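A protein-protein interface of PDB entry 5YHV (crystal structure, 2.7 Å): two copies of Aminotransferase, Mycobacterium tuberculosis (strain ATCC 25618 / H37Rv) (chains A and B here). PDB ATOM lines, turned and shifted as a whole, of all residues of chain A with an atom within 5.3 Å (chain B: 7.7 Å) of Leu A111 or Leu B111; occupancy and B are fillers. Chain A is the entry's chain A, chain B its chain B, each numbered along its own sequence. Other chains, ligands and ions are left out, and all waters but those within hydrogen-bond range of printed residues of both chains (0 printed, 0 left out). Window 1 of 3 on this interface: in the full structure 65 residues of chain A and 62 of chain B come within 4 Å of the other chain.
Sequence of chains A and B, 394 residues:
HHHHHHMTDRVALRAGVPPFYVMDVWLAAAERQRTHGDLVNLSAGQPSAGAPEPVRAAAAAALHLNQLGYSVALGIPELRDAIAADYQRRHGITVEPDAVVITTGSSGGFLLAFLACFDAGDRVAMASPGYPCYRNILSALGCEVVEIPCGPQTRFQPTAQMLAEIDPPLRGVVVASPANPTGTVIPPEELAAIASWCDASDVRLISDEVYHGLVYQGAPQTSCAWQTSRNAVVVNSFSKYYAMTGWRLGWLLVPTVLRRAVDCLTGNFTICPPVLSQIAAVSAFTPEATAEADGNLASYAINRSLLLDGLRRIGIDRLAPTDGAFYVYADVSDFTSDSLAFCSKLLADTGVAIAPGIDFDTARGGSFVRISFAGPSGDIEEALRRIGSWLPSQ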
ATOM      1  N   SER A 106      12.318   1.656  -3.730  1.00  0.00           N
ATOM      2  CA  SER A 106      13.072   2.833  -4.154  1.00  0.00           C
ATOM      3  C   SER A 106      14.190   2.437  -5.124  1.00  0.00           C
ATOM      4  O   SER A 106      14.555   3.223  -5.996  1.00  0.00           O
ATOM      5  CB  SER A 106      13.606   3.628  -2.962  1.00  0.00           C
ATOM      6  OG  SER A 106      14.557   2.892  -2.230  1.00  0.00           O
ATOM      7  N   SER A 107      14.697   1.208  -4.977  1.00  0.00           N
ATOM      8  CA  SER A 107      15.650   0.604  -5.920  1.00  0.00           C
ATOM      9  C   SER A 107      15.131   0.596  -7.355  1.00  0.00           C
ATOM     10  O   SER A 107      15.884   0.885  -8.288  1.00  0.00           O
ATOM     11  CB  SER A 107      15.998  -0.822  -5.496  1.00  0.00           C
ATOM     12  OG  SER A 107      16.670  -0.823  -4.252  1.00  0.00           O
ATOM     13  N   GLY A 108      13.849   0.261  -7.519  1.00  0.00           N
ATOM     14  CA  GLY A 108      13.172   0.339  -8.811  1.00  0.00           C
ATOM     15  C   GLY A 108      12.992   1.780  -9.247  1.00  0.00           C
ATOM     16  O   GLY A 108      13.110   2.090 -10.439  1.00  0.00           O
ATOM     17  N   GLY A 109      12.715   2.650  -8.271  1.00  0.00           N
ATOM     18  CA  GLY A 109      12.571   4.089  -8.486  1.00  0.00           C
ATOM     19  C   GLY A 109      13.839   4.753  -8.991  1.00  0.00           C
ATOM     20  O   GLY A 109      13.772   5.603  -9.889  1.00  0.00           O
ATOM     21  N   PHE A 110      14.984   4.357  -8.424  1.00  0.00           N
ATOM     22  CA  PHE A 110      16.297   4.854  -8.862  1.00  0.00           C
ATOM     23  C   PHE A 110      16.627   4.447 -10.290  1.00  0.00           C
ATOM     24  O   PHE A 110      17.171   5.254 -11.043  1.00  0.00           O
ATOM     25  CB  PHE A 110      17.425   4.443  -7.897  1.00  0.00           C
ATOM     26  CG  PHE A 110      17.459   5.246  -6.626  1.00  0.00           C
ATOM     27  CD1 PHE A 110      17.703   6.622  -6.654  1.00  0.00           C
ATOM     28  CD2 PHE A 110      17.255   4.632  -5.392  1.00  0.00           C
ATOM     29  CE1 PHE A 110      17.732   7.371  -5.481  1.00  0.00           C
ATOM     30  CE2 PHE A 110      17.277   5.373  -4.216  1.00  0.00           C
ATOM     31  CZ  PHE A 110      17.510   6.745  -4.266  1.00  0.00           C
ATOM     32  N   LEU A 111      16.291   3.210 -10.657  1.00  0.00           N
ATOM     33  CA  LEU A 111      16.460   2.724 -12.029  1.00  0.00           C
ATOM     34  C   LEU A 111      15.696   3.595 -13.028  1.00  0.00           C
ATOM     35  O   LEU A 111      16.243   3.976 -14.065  1.00  0.00           O
ATOM     36  CB  LEU A 111      16.035   1.251 -12.157  1.00  0.00           C
ATOM     37  CG  LEU A 111      15.975   0.613 -13.550  1.00  0.00           C
ATOM     38  CD1 LEU A 111      17.365   0.372 -14.137  1.00  0.00           C
ATOM     39  CD2 LEU A 111      15.186  -0.689 -13.505  1.00  0.00           C
ATOM     40  N   LEU A 112      14.442   3.913 -12.698  1.00  0.00           N
ATOM     41  CA  LEU A 112      13.605   4.771 -13.532  1.00  0.00           C
ATOM     42  C   LEU A 112      14.131   6.200 -13.570  1.00  0.00           C
ATOM     43  O   LEU A 112      14.248   6.780 -14.647  1.00  0.00           O
ATOM     44  CB  LEU A 112      12.144   4.746 -13.066  1.00  0.00           C
ATOM     45  CG  LEU A 112      11.369   3.424 -13.087  1.00  0.00           C
ATOM     46  CD1 LEU A 112       9.990   3.623 -12.475  1.00  0.00           C
ATOM     47  CD2 LEU A 112      11.261   2.848 -14.489  1.00  0.00           C
ATOM     48  N   ALA A 113      14.459   6.743 -12.396  1.00  0.00           N
ATOM     49  CA  ALA A 113      14.982   8.106 -12.269  1.00  0.00           C
ATOM     50  C   ALA A 113      16.272   8.310 -13.060  1.00  0.00           C
ATOM     51  O   ALA A 113      16.399   9.296 -13.778  1.00  0.00           O
ATOM     52  CB  ALA A 113      15.181   8.473 -10.806  1.00  0.00           C
ATOM     53  N   PHE A 114      17.204   7.365 -12.952  1.00  0.00           N
ATOM     54  CA  PHE A 114      18.496   7.479 -13.635  1.00  0.00           C
ATOM     55  C   PHE A 114      18.394   7.327 -15.158  1.00  0.00           C
ATOM     56  O   PHE A 114      19.094   8.025 -15.896  1.00  0.00           O
ATOM     57  CB  PHE A 114      19.537   6.513 -13.048  1.00  0.00           C
ATOM     58  CG  PHE A 114      19.890   6.780 -11.600  1.00  0.00           C
ATOM     59  CD1 PHE A 114      19.735   8.054 -11.026  1.00  0.00           C
ATOM     60  CD2 PHE A 114      20.412   5.754 -10.804  1.00  0.00           C
ATOM     61  CE1 PHE A 114      20.068   8.284  -9.696  1.00  0.00           C
ATOM     62  CE2 PHE A 114      20.751   5.989  -9.471  1.00  0.00           C
ATOM     63  CZ  PHE A 114      20.581   7.252  -8.922  1.00  0.00           C
ATOM     64  N   LEU A 115      17.519   6.432 -15.615  1.00  0.00           N
ATOM     65  CA  LEU A 115      17.280   6.227 -17.052  1.00  0.00           C
ATOM     66  C   LEU A 115      16.522   7.389 -17.704  1.00  0.00           C
ATOM     67  O   LEU A 115      16.788   7.732 -18.859  1.00  0.00           O
ATOM     68  CB  LEU A 115      16.554   4.899 -17.327  1.00  0.00           C
ATOM     69  CG  LEU A 115      17.325   3.571 -17.187  1.00  0.00           C
ATOM     70  CD1 LEU A 115      16.360   2.400 -17.275  1.00  0.00           C
ATOM     71  CD2 LEU A 115      18.458   3.404 -18.195  1.00  0.00           C
ATOM     72  N   ALA A 116      15.584   7.981 -16.964  1.00  0.00           N
ATOM     73  CA  ALA A 116      14.778   9.098 -17.467  1.00  0.00           C
ATOM     74  C   ALA A 116      15.538  10.423 -17.482  1.00  0.00           C
ATOM     75  O   ALA A 116      15.344  11.238 -18.387  1.00  0.00           O
ATOM     76  CB  ALA A 116      13.482   9.231 -16.679  1.00  0.00           C
ATOM     77  N   ILE A 137      24.606   1.378  -9.450  1.00  0.00           N
ATOM     78  CA  ILE A 137      23.540   1.477 -10.458  1.00  0.00           C
ATOM     79  C   ILE A 137      23.966   2.437 -11.575  1.00  0.00           C
ATOM     80  O   ILE A 137      23.907   2.080 -12.752  1.00  0.00           O
ATOM     81  CB  ILE A 137      22.160   1.867  -9.852  1.00  0.00           C
ATOM     82  CG1 ILE A 137      21.604   0.724  -8.991  1.00  0.00           C
ATOM     83  CG2 ILE A 137      21.145   2.208 -10.945  1.00  0.00           C
ATOM     84  CD1 ILE A 137      20.528   1.148  -8.012  1.00  0.00           C
ATOM     85  N   LEU A 141      24.742   1.655 -15.501  1.00  0.00           N
ATOM     86  CA  LEU A 141      23.946   2.369 -16.507  1.00  0.00           C
ATOM     87  C   LEU A 141      24.784   3.344 -17.356  1.00  0.00           C
ATOM     88  O   LEU A 141      24.231   4.115 -18.144  1.00  0.00           O
ATOM     89  CB  LEU A 141      22.739   3.075 -15.868  1.00  0.00           C
ATOM     90  CG  LEU A 141      21.621   2.253 -15.202  1.00  0.00           C
ATOM     91  CD1 LEU A 141      20.550   3.173 -14.650  1.00  0.00           C
ATOM     92  CD2 LEU A 141      20.984   1.220 -16.124  1.00  0.00           C
ATOM     93  N   PHE A 269      10.110  -1.991 -18.451  1.00  0.00           N
ATOM     94  CA  PHE A 269      11.074  -2.582 -17.521  1.00  0.00           C
ATOM     95  C   PHE A 269      10.476  -3.442 -16.408  1.00  0.00           C
ATOM     96  O   PHE A 269      11.093  -4.436 -16.009  1.00  0.00           O
ATOM     97  CB  PHE A 269      11.979  -1.502 -16.915  1.00  0.00           C
ATOM     98  CG  PHE A 269      13.150  -1.137 -17.782  1.00  0.00           C
ATOM     99  CD1 PHE A 269      13.014  -0.202 -18.809  1.00  0.00           C
ATOM    100  CD2 PHE A 269      14.398  -1.725 -17.571  1.00  0.00           C
ATOM    101  CE1 PHE A 269      14.097   0.134 -19.611  1.00  0.00           C
ATOM    102  CE2 PHE A 269      15.487  -1.392 -18.372  1.00  0.00           C
ATOM    103  CZ  PHE A 269      15.335  -0.467 -19.397  1.00  0.00           C
ATOM    104  N   ARG B  14      17.973   8.339 -24.356  1.00  0.00           N
ATOM    105  CA  ARG B  14      17.720   6.900 -24.166  1.00  0.00           C
ATOM    106  C   ARG B  14      16.350   6.600 -23.547  1.00  0.00           C
ATOM    107  O   ARG B  14      15.791   5.520 -23.764  1.00  0.00           O
ATOM    108  CB  ARG B  14      18.834   6.243 -23.332  1.00  0.00           C
ATOM    109  CG  ARG B  14      19.070   6.865 -21.953  1.00  0.00           C
ATOM    110  CD  ARG B  14      19.283   5.827 -20.846  1.00  0.00           C
ATOM    111  NE  ARG B  14      20.686   5.498 -20.540  1.00  0.00           N
ATOM    112  CZ  ARG B  14      21.279   5.655 -19.352  1.00  0.00           C
ATOM    113  NH1 ARG B  14      22.545   5.321 -19.216  1.00  0.00           N
ATOM    114  NH2 ARG B  14      20.616   6.148 -18.314  1.00  0.00           N
ATOM    115  N   THR B 103      14.058 -13.666  -9.734  1.00  0.00           N
ATOM    116  CA  THR B 103      13.982 -12.292 -10.250  1.00  0.00           C
ATOM    117  C   THR B 103      12.587 -11.684 -10.048  1.00  0.00           C
ATOM    118  O   THR B 103      11.601 -12.418  -9.886  1.00  0.00           O
ATOM    119  CB  THR B 103      14.343 -12.221 -11.754  1.00  0.00           C
ATOM    120  OG1 THR B 103      13.391 -12.972 -12.517  1.00  0.00           O
ATOM    121  CG2 THR B 103      15.744 -12.773 -12.031  1.00  0.00           C
ATOM    122  N   GLY B 105       9.850 -10.784 -11.584  1.00  0.00           N
ATOM    123  CA  GLY B 105       9.282 -11.112 -12.886  1.00  0.00           C
ATOM    124  C   GLY B 105      10.359 -11.455 -13.904  1.00  0.00           C
ATOM    125  O   GLY B 105      11.557 -11.353 -13.619  1.00  0.00           O
ATOM    126  N   SER B 106       9.937 -11.877 -15.093  1.00  0.00           N
ATOM    127  CA  SER B 106      10.859 -12.061 -16.206  1.00  0.00           C
ATOM    128  C   SER B 106      11.380 -10.711 -16.714  1.00  0.00           C
ATOM    129  O   SER B 106      12.507 -10.632 -17.198  1.00  0.00           O
ATOM    130  CB  SER B 106      10.228 -12.891 -17.325  1.00  0.00           C
ATOM    131  OG  SER B 106       9.147 -12.219 -17.927  1.00  0.00           O
ATOM    132  N   SER B 107      10.566  -9.663 -16.564  1.00  0.00           N
ATOM    133  CA  SER B 107      10.963  -8.273 -16.823  1.00  0.00           C
ATOM    134  C   SER B 107      12.213  -7.860 -16.049  1.00  0.00           C
ATOM    135  O   SER B 107      13.096  -7.198 -16.598  1.00  0.00           O
ATOM    136  CB  SER B 107       9.817  -7.319 -16.486  1.00  0.00           C
ATOM    137  OG  SER B 107       8.714  -7.540 -17.340  1.00  0.00           O
ATOM    138  N   GLY B 108      12.271  -8.250 -14.776  1.00  0.00           N
ATOM    139  CA  GLY B 108      13.450  -8.051 -13.939  1.00  0.00           C
ATOM    140  C   GLY B 108      14.597  -8.929 -14.396  1.00  0.00           C
ATOM    141  O   GLY B 108      15.757  -8.511 -14.358  1.00  0.00           O
ATOM    142  N   GLY B 109      14.257 -10.142 -14.835  1.00  0.00           N
ATOM    143  CA  GLY B 109      15.213 -11.107 -15.378  1.00  0.00           C
ATOM    144  C   GLY B 109      15.899 -10.627 -16.642  1.00  0.00           C
ATOM    145  O   GLY B 109      17.111 -10.817 -16.793  1.00  0.00           O
ATOM    146  N   PHE B 110      15.128  -9.999 -17.536  1.00  0.00           N
ATOM    147  CA  PHE B 110      15.665  -9.412 -18.771  1.00  0.00           C
ATOM    148  C   PHE B 110      16.634  -8.267 -18.502  1.00  0.00           C
ATOM    149  O   PHE B 110      17.663  -8.166 -19.171  1.00  0.00           O
ATOM    150  CB  PHE B 110      14.553  -8.980 -19.746  1.00  0.00           C
ATOM    151  CG  PHE B 110      13.907 -10.129 -20.477  1.00  0.00           C
ATOM    152  CD1 PHE B 110      14.651 -10.936 -21.347  1.00  0.00           C
ATOM    153  CD2 PHE B 110      12.550 -10.410 -20.297  1.00  0.00           C
ATOM    154  CE1 PHE B 110      14.062 -12.005 -22.005  1.00  0.00           C
ATOM    155  CE2 PHE B 110      11.952 -11.481 -20.956  1.00  0.00           C
ATOM    156  CZ  PHE B 110      12.711 -12.282 -21.809  1.00  0.00           C
ATOM    157  N   LEU B 111      16.309  -7.427 -17.514  1.00  0.00           N
ATOM    158  CA  LEU B 111      17.196  -6.346 -17.078  1.00  0.00           C
ATOM    159  C   LEU B 111      18.560  -6.888 -16.634  1.00  0.00           C
ATOM    160  O   LEU B 111      19.598  -6.354 -17.026  1.00  0.00           O
ATOM    161  CB  LEU B 111      16.551  -5.515 -15.958  1.00  0.00           C
ATOM    162  CG  LEU B 111      17.406  -4.453 -15.234  1.00  0.00           C
ATOM    163  CD1 LEU B 111      17.681  -3.235 -16.110  1.00  0.00           C
ATOM    164  CD2 LEU B 111      16.776  -4.058 -13.905  1.00  0.00           C
ATOM    165  N   LEU B 112      18.540  -7.953 -15.832  1.00  0.00           N
ATOM    166  CA  LEU B 112      19.759  -8.599 -15.356  1.00  0.00           C
ATOM    167  C   LEU B 112      20.513  -9.273 -16.490  1.00  0.00           C
ATOM    168  O   LEU B 112      21.726  -9.087 -16.616  1.00  0.00           O
ATOM    169  CB  LEU B 112      19.456  -9.605 -14.236  1.00  0.00           C
ATOM    170  CG  LEU B 112      18.832  -9.097 -12.928  1.00  0.00           C
ATOM    171  CD1 LEU B 112      18.524 -10.274 -12.017  1.00  0.00           C
ATOM    172  CD2 LEU B 112      19.713  -8.073 -12.217  1.00  0.00           C
ATOM    173  N   ALA B 113      19.787 -10.029 -17.319  1.00  0.00           N
ATOM    174  CA  ALA B 113      20.368 -10.742 -18.458  1.00  0.00           C
ATOM    175  C   ALA B 113      21.055  -9.796 -19.442  1.00  0.00           C
ATOM    176  O   ALA B 113      22.176 -10.059 -19.865  1.00  0.00           O
ATOM    177  CB  ALA B 113      19.314 -11.580 -19.164  1.00  0.00           C
ATOM    178  N   PHE B 114      20.395  -8.685 -19.780  1.00  0.00           N
ATOM    179  CA  PHE B 114      20.939  -7.735 -20.750  1.00  0.00           C
ATOM    180  C   PHE B 114      22.145  -6.957 -20.226  1.00  0.00           C
ATOM    181  O   PHE B 114      23.090  -6.703 -20.985  1.00  0.00           O
ATOM    182  CB  PHE B 114      19.857  -6.790 -21.290  1.00  0.00           C
ATOM    183  CG  PHE B 114      18.753  -7.483 -22.066  1.00  0.00           C
ATOM    184  CD1 PHE B 114      18.957  -8.717 -22.699  1.00  0.00           C
ATOM    185  CD2 PHE B 114      17.507  -6.873 -22.195  1.00  0.00           C
ATOM    186  CE1 PHE B 114      17.935  -9.332 -23.412  1.00  0.00           C
ATOM    187  CE2 PHE B 114      16.482  -7.479 -22.910  1.00  0.00           C
ATOM    188  CZ  PHE B 114      16.696  -8.710 -23.522  1.00  0.00           C
ATOM    189  N   LEU B 115      22.114  -6.592 -18.939  1.00  0.00           N
ATOM    190  CA  LEU B 115      23.236  -5.895 -18.296  1.00  0.00           C
ATOM    191  C   LEU B 115      24.460  -6.790 -18.085  1.00  0.00           C
ATOM    192  O   LEU B 115      25.599  -6.323 -18.206  1.00  0.00           O
ATOM    193  CB  LEU B 115      22.818  -5.252 -16.966  1.00  0.00           C
ATOM    194  CG  LEU B 115      21.947  -3.996 -16.939  1.00  0.00           C
ATOM    195  CD1 LEU B 115      21.480  -3.707 -15.519  1.00  0.00           C
ATOM    196  CD2 LEU B 115      22.652  -2.779 -17.532  1.00  0.00           C
ATOM    197  N   ALA B 116      24.220  -8.066 -17.769  1.00  0.00           N
ATOM    198  CA  ALA B 116      25.299  -9.027 -17.529  1.00  0.00           C
ATOM    199  C   ALA B 116      25.959  -9.518 -18.815  1.00  0.00           C
ATOM    200  O   ALA B 116      27.171  -9.749 -18.839  1.00  0.00           O
ATOM    201  CB  ALA B 116      24.803 -10.202 -16.699  1.00  0.00           C
ATOM    202  N   CYS B 117      25.166  -9.659 -19.877  1.00  0.00           N
ATOM    203  CA  CYS B 117      25.637 -10.243 -21.138  1.00  0.00           C
ATOM    204  C   CYS B 117      26.170  -9.240 -22.150  1.00  0.00           C
ATOM    205  O   CYS B 117      27.098  -9.557 -22.897  1.00  0.00           O
ATOM    206  CB  CYS B 117      24.535 -11.074 -21.793  1.00  0.00           C
ATOM    207  SG  CYS B 117      24.011 -12.488 -20.808  1.00  0.00           S
ATOM    208  N   ILE B 137      13.796  -2.250 -23.810  1.00  0.00           N
ATOM    209  CA  ILE B 137      14.783  -2.415 -22.731  1.00  0.00           C
ATOM    210  C   ILE B 137      16.198  -2.298 -23.307  1.00  0.00           C
ATOM    211  O   ILE B 137      17.007  -1.509 -22.803  1.00  0.00           O
ATOM    212  CB  ILE B 137      14.595  -3.730 -21.921  1.00  0.00           C
ATOM    213  CG1 ILE B 137      13.308  -3.680 -21.088  1.00  0.00           C
ATOM    214  CG2 ILE B 137      15.763  -3.959 -20.972  1.00  0.00           C
ATOM    215  CD1 ILE B 137      12.797  -5.037 -20.640  1.00  0.00           C
ATOM    216  N   LEU B 141      19.032   0.564 -22.646  1.00  0.00           N
ATOM    217  CA  LEU B 141      20.324   0.129 -22.102  1.00  0.00           C
ATOM    218  C   LEU B 141      21.490   0.317 -23.088  1.00  0.00           C
ATOM    219  O   LEU B 141      22.608  -0.144 -22.829  1.00  0.00           O
ATOM    220  CB  LEU B 141      20.251  -1.323 -21.592  1.00  0.00           C
ATOM    221  CG  LEU B 141      19.340  -1.683 -20.401  1.00  0.00           C
ATOM    222  CD1 LEU B 141      19.447  -3.162 -20.096  1.00  0.00           C
ATOM    223  CD2 LEU B 141      19.617  -0.868 -19.142  1.00  0.00           C
ATOM    224  N   VAL B 235      15.129 -17.505 -19.547  1.00  0.00           N
ATOM    225  CA  VAL B 235      14.253 -16.584 -18.835  1.00  0.00           C
ATOM    226  C   VAL B 235      12.880 -17.241 -18.719  1.00  0.00           C
ATOM    227  O   VAL B 235      12.330 -17.732 -19.709  1.00  0.00           O
ATOM    228  CB  VAL B 235      14.151 -15.209 -19.540  1.00  0.00           C
ATOM    229  CG1 VAL B 235      13.428 -14.197 -18.658  1.00  0.00           C
ATOM    230  CG2 VAL B 235      15.530 -14.676 -19.911  1.00  0.00           C
ATOM    231  N   LEU B 252      15.804 -16.987 -13.621  1.00  0.00           N
ATOM    232  CA  LEU B 252      16.775 -17.196 -14.683  1.00  0.00           C
ATOM    233  C   LEU B 252      17.559 -18.475 -14.433  1.00  0.00           C
ATOM    234  O   LEU B 252      17.849 -18.809 -13.284  1.00  0.00           O
ATOM    235  CB  LEU B 252      17.771 -16.033 -14.748  1.00  0.00           C
ATOM    236  CG  LEU B 252      17.356 -14.589 -15.013  1.00  0.00           C
ATOM    237  CD1 LEU B 252      18.515 -13.673 -14.655  1.00  0.00           C
ATOM    238  CD2 LEU B 252      16.931 -14.376 -16.457  1.00  0.00           C
ATOM    239  N   LEU B 265      24.726  -7.442  -9.742  1.00  0.00           N
ATOM    240  CA  LEU B 265      23.733  -6.555 -10.347  1.00  0.00           C
ATOM    241  C   LEU B 265      22.399  -6.600  -9.608  1.00  0.00           C
ATOM    242  O   LEU B 265      21.834  -5.549  -9.303  1.00  0.00           O
ATOM    243  CB  LEU B 265      23.549  -6.853 -11.843  1.00  0.00           C
ATOM    244  CG  LEU B 265      24.671  -6.451 -12.812  1.00  0.00           C
ATOM    245  CD1 LEU B 265      24.558  -7.239 -14.112  1.00  0.00           C
ATOM    246  CD2 LEU B 265      24.710  -4.954 -13.089  1.00  0.00           C
ATOM    247  N   THR B 266      21.922  -7.807  -9.295  1.00  0.00           N
ATOM    248  CA  THR B 266      20.614  -7.983  -8.652  1.00  0.00           C
ATOM    249  C   THR B 266      20.528  -7.352  -7.256  1.00  0.00           C
ATOM    250  O   THR B 266      19.519  -6.723  -6.924  1.00  0.00           O
ATOM    251  CB  THR B 266      20.106  -9.454  -8.693  1.00  0.00           C
ATOM    252  OG1 THR B 266      18.697  -9.483  -8.435  1.00  0.00           O
ATOM    253  CG2 THR B 266      20.835 -10.374  -7.711  1.00  0.00           C
ATOM    254  N   PHE B 269      20.562  -3.451  -7.918  1.00  0.00           N
ATOM    255  CA  PHE B 269      19.401  -2.961  -8.665  1.00  0.00           C
ATOM    256  C   PHE B 269      18.044  -3.230  -8.018  1.00  0.00           C
ATOM    257  O   PHE B 269      17.135  -2.402  -8.144  1.00  0.00           O
ATOM    258  CB  PHE B 269      19.413  -3.495 -10.101  1.00  0.00           C
ATOM    259  CG  PHE B 269      20.270  -2.695 -11.039  1.00  0.00           C
ATOM    260  CD1 PHE B 269      21.648  -2.923 -11.123  1.00  0.00           C
ATOM    261  CD2 PHE B 269      19.705  -1.710 -11.848  1.00  0.00           C
ATOM    262  CE1 PHE B 269      22.442  -2.181 -11.986  1.00  0.00           C
ATOM    263  CE2 PHE B 269      20.492  -0.965 -12.721  1.00  0.00           C
ATOM    264  CZ  PHE B 269      21.862  -1.204 -12.794  1.00  0.00           C
ATOM    265  N   THR B 270      17.904  -4.377  -7.345  1.00  0.00           N
ATOM    266  CA  THR B 270      16.609  -4.815  -6.787  1.00  0.00           C
ATOM    267  C   THR B 270      16.640  -5.143  -5.286  1.00  0.00           C
ATOM    268  O   THR B 270      15.583  -5.225  -4.647  1.00  0.00           O
ATOM    269  CB  THR B 270      16.018  -6.045  -7.536  1.00  0.00           C
ATOM    270  OG1 THR B 270      16.782  -7.226  -7.241  1.00  0.00           O
ATOM    271  CG2 THR B 270      15.959  -5.825  -9.058  1.00  0.00           C
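Ser A107 touches Phe B269, and with the chains exchanged Phe A269 touches Ser B107. Leu B111 touches its own counterpart, Leu A111. Leu A111 touches Phe B269, and with the chains exchanged Phe A269 touches Leu B111. Ile A137 touches Phe B269, and with the chains exchanged Phe A269 touches Ile B137.
Of the printed residues of chain B, Ser A107 touches Phe B269. Leu A111 touches just these residues of chain B: Leu B111 (3.7 Å) and Phe B269 (3.7 Å). Of the printed residues of chain B, Leu A115 touches Arg B14. Printed residues of chain B within 4 Å of Ile A137: Phe B269. Of the printed residues of chain A, Arg B14 touches Phe A114, Leu A115 and Leu A141. Thr B103 touches none of the printed residues of chain A. Of chain A, only Leu A111 (3.7 Å) and Phe A269 (3.7 Å) come within 4 Å of Leu B111. Printed residues of chain A within 4 Å of Phe B269: Ser A107 (3.3 Å), Leu A111 (3.7 Å) and Ile A137 (3.7 Å). The nearest residue of chain B that does not touch Leu A111 is Leu B141 (5.6 Å). The nearest printed residue of chain A that does not touch Leu B111 is Leu A141 (5.5 Å). The nearest printed residue of chain A that does not touch Ser B107 is Leu A111 (7.5 Å).
Along chain A the printed residues that touch a printed residue of chain B span positions 107 to 269. Hydrophobic or aromatic side chains of chain B that line the printed part of chain A: Leu B111, Ile B137, Leu B141 and Phe B269. Among the printed residues, 11 pairs touch across the chains. Among the printed residues, no Asp or Glu carboxylate lies within 4 Å of a Lys or Arg side-chain nitrogen of the other chain.
Phe B269 touches Ser A107 (O to CB, 3.3 Å). CD2 of Leu B111 touches CD2 of Leu A111 (3.7 Å). Phe B269 touches Leu A111. Arg B14 touches Leu A115. Phe B269 touches Ile A137. Leu A141 touches Leu B141 (CD2 to CD2, 3.9 Å). CE2 of Phe A269 touches CD1 of Leu B111, at 3.7 Å. Ile B137 touches Phe A269 (CG2 to CE2, 3.7 Å).
The backbone carbonyl oxygen of Phe A269 sits close to the backbone carbonyl oxygen of Ser B107, 3.5 Å away. NH2 of Arg B14 lies within hydrogen-bond range of O of Phe A114. The backbone carbonyl oxygen of Leu A141 sits close to the guanidinium group of Arg B14 (2.3 Å).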
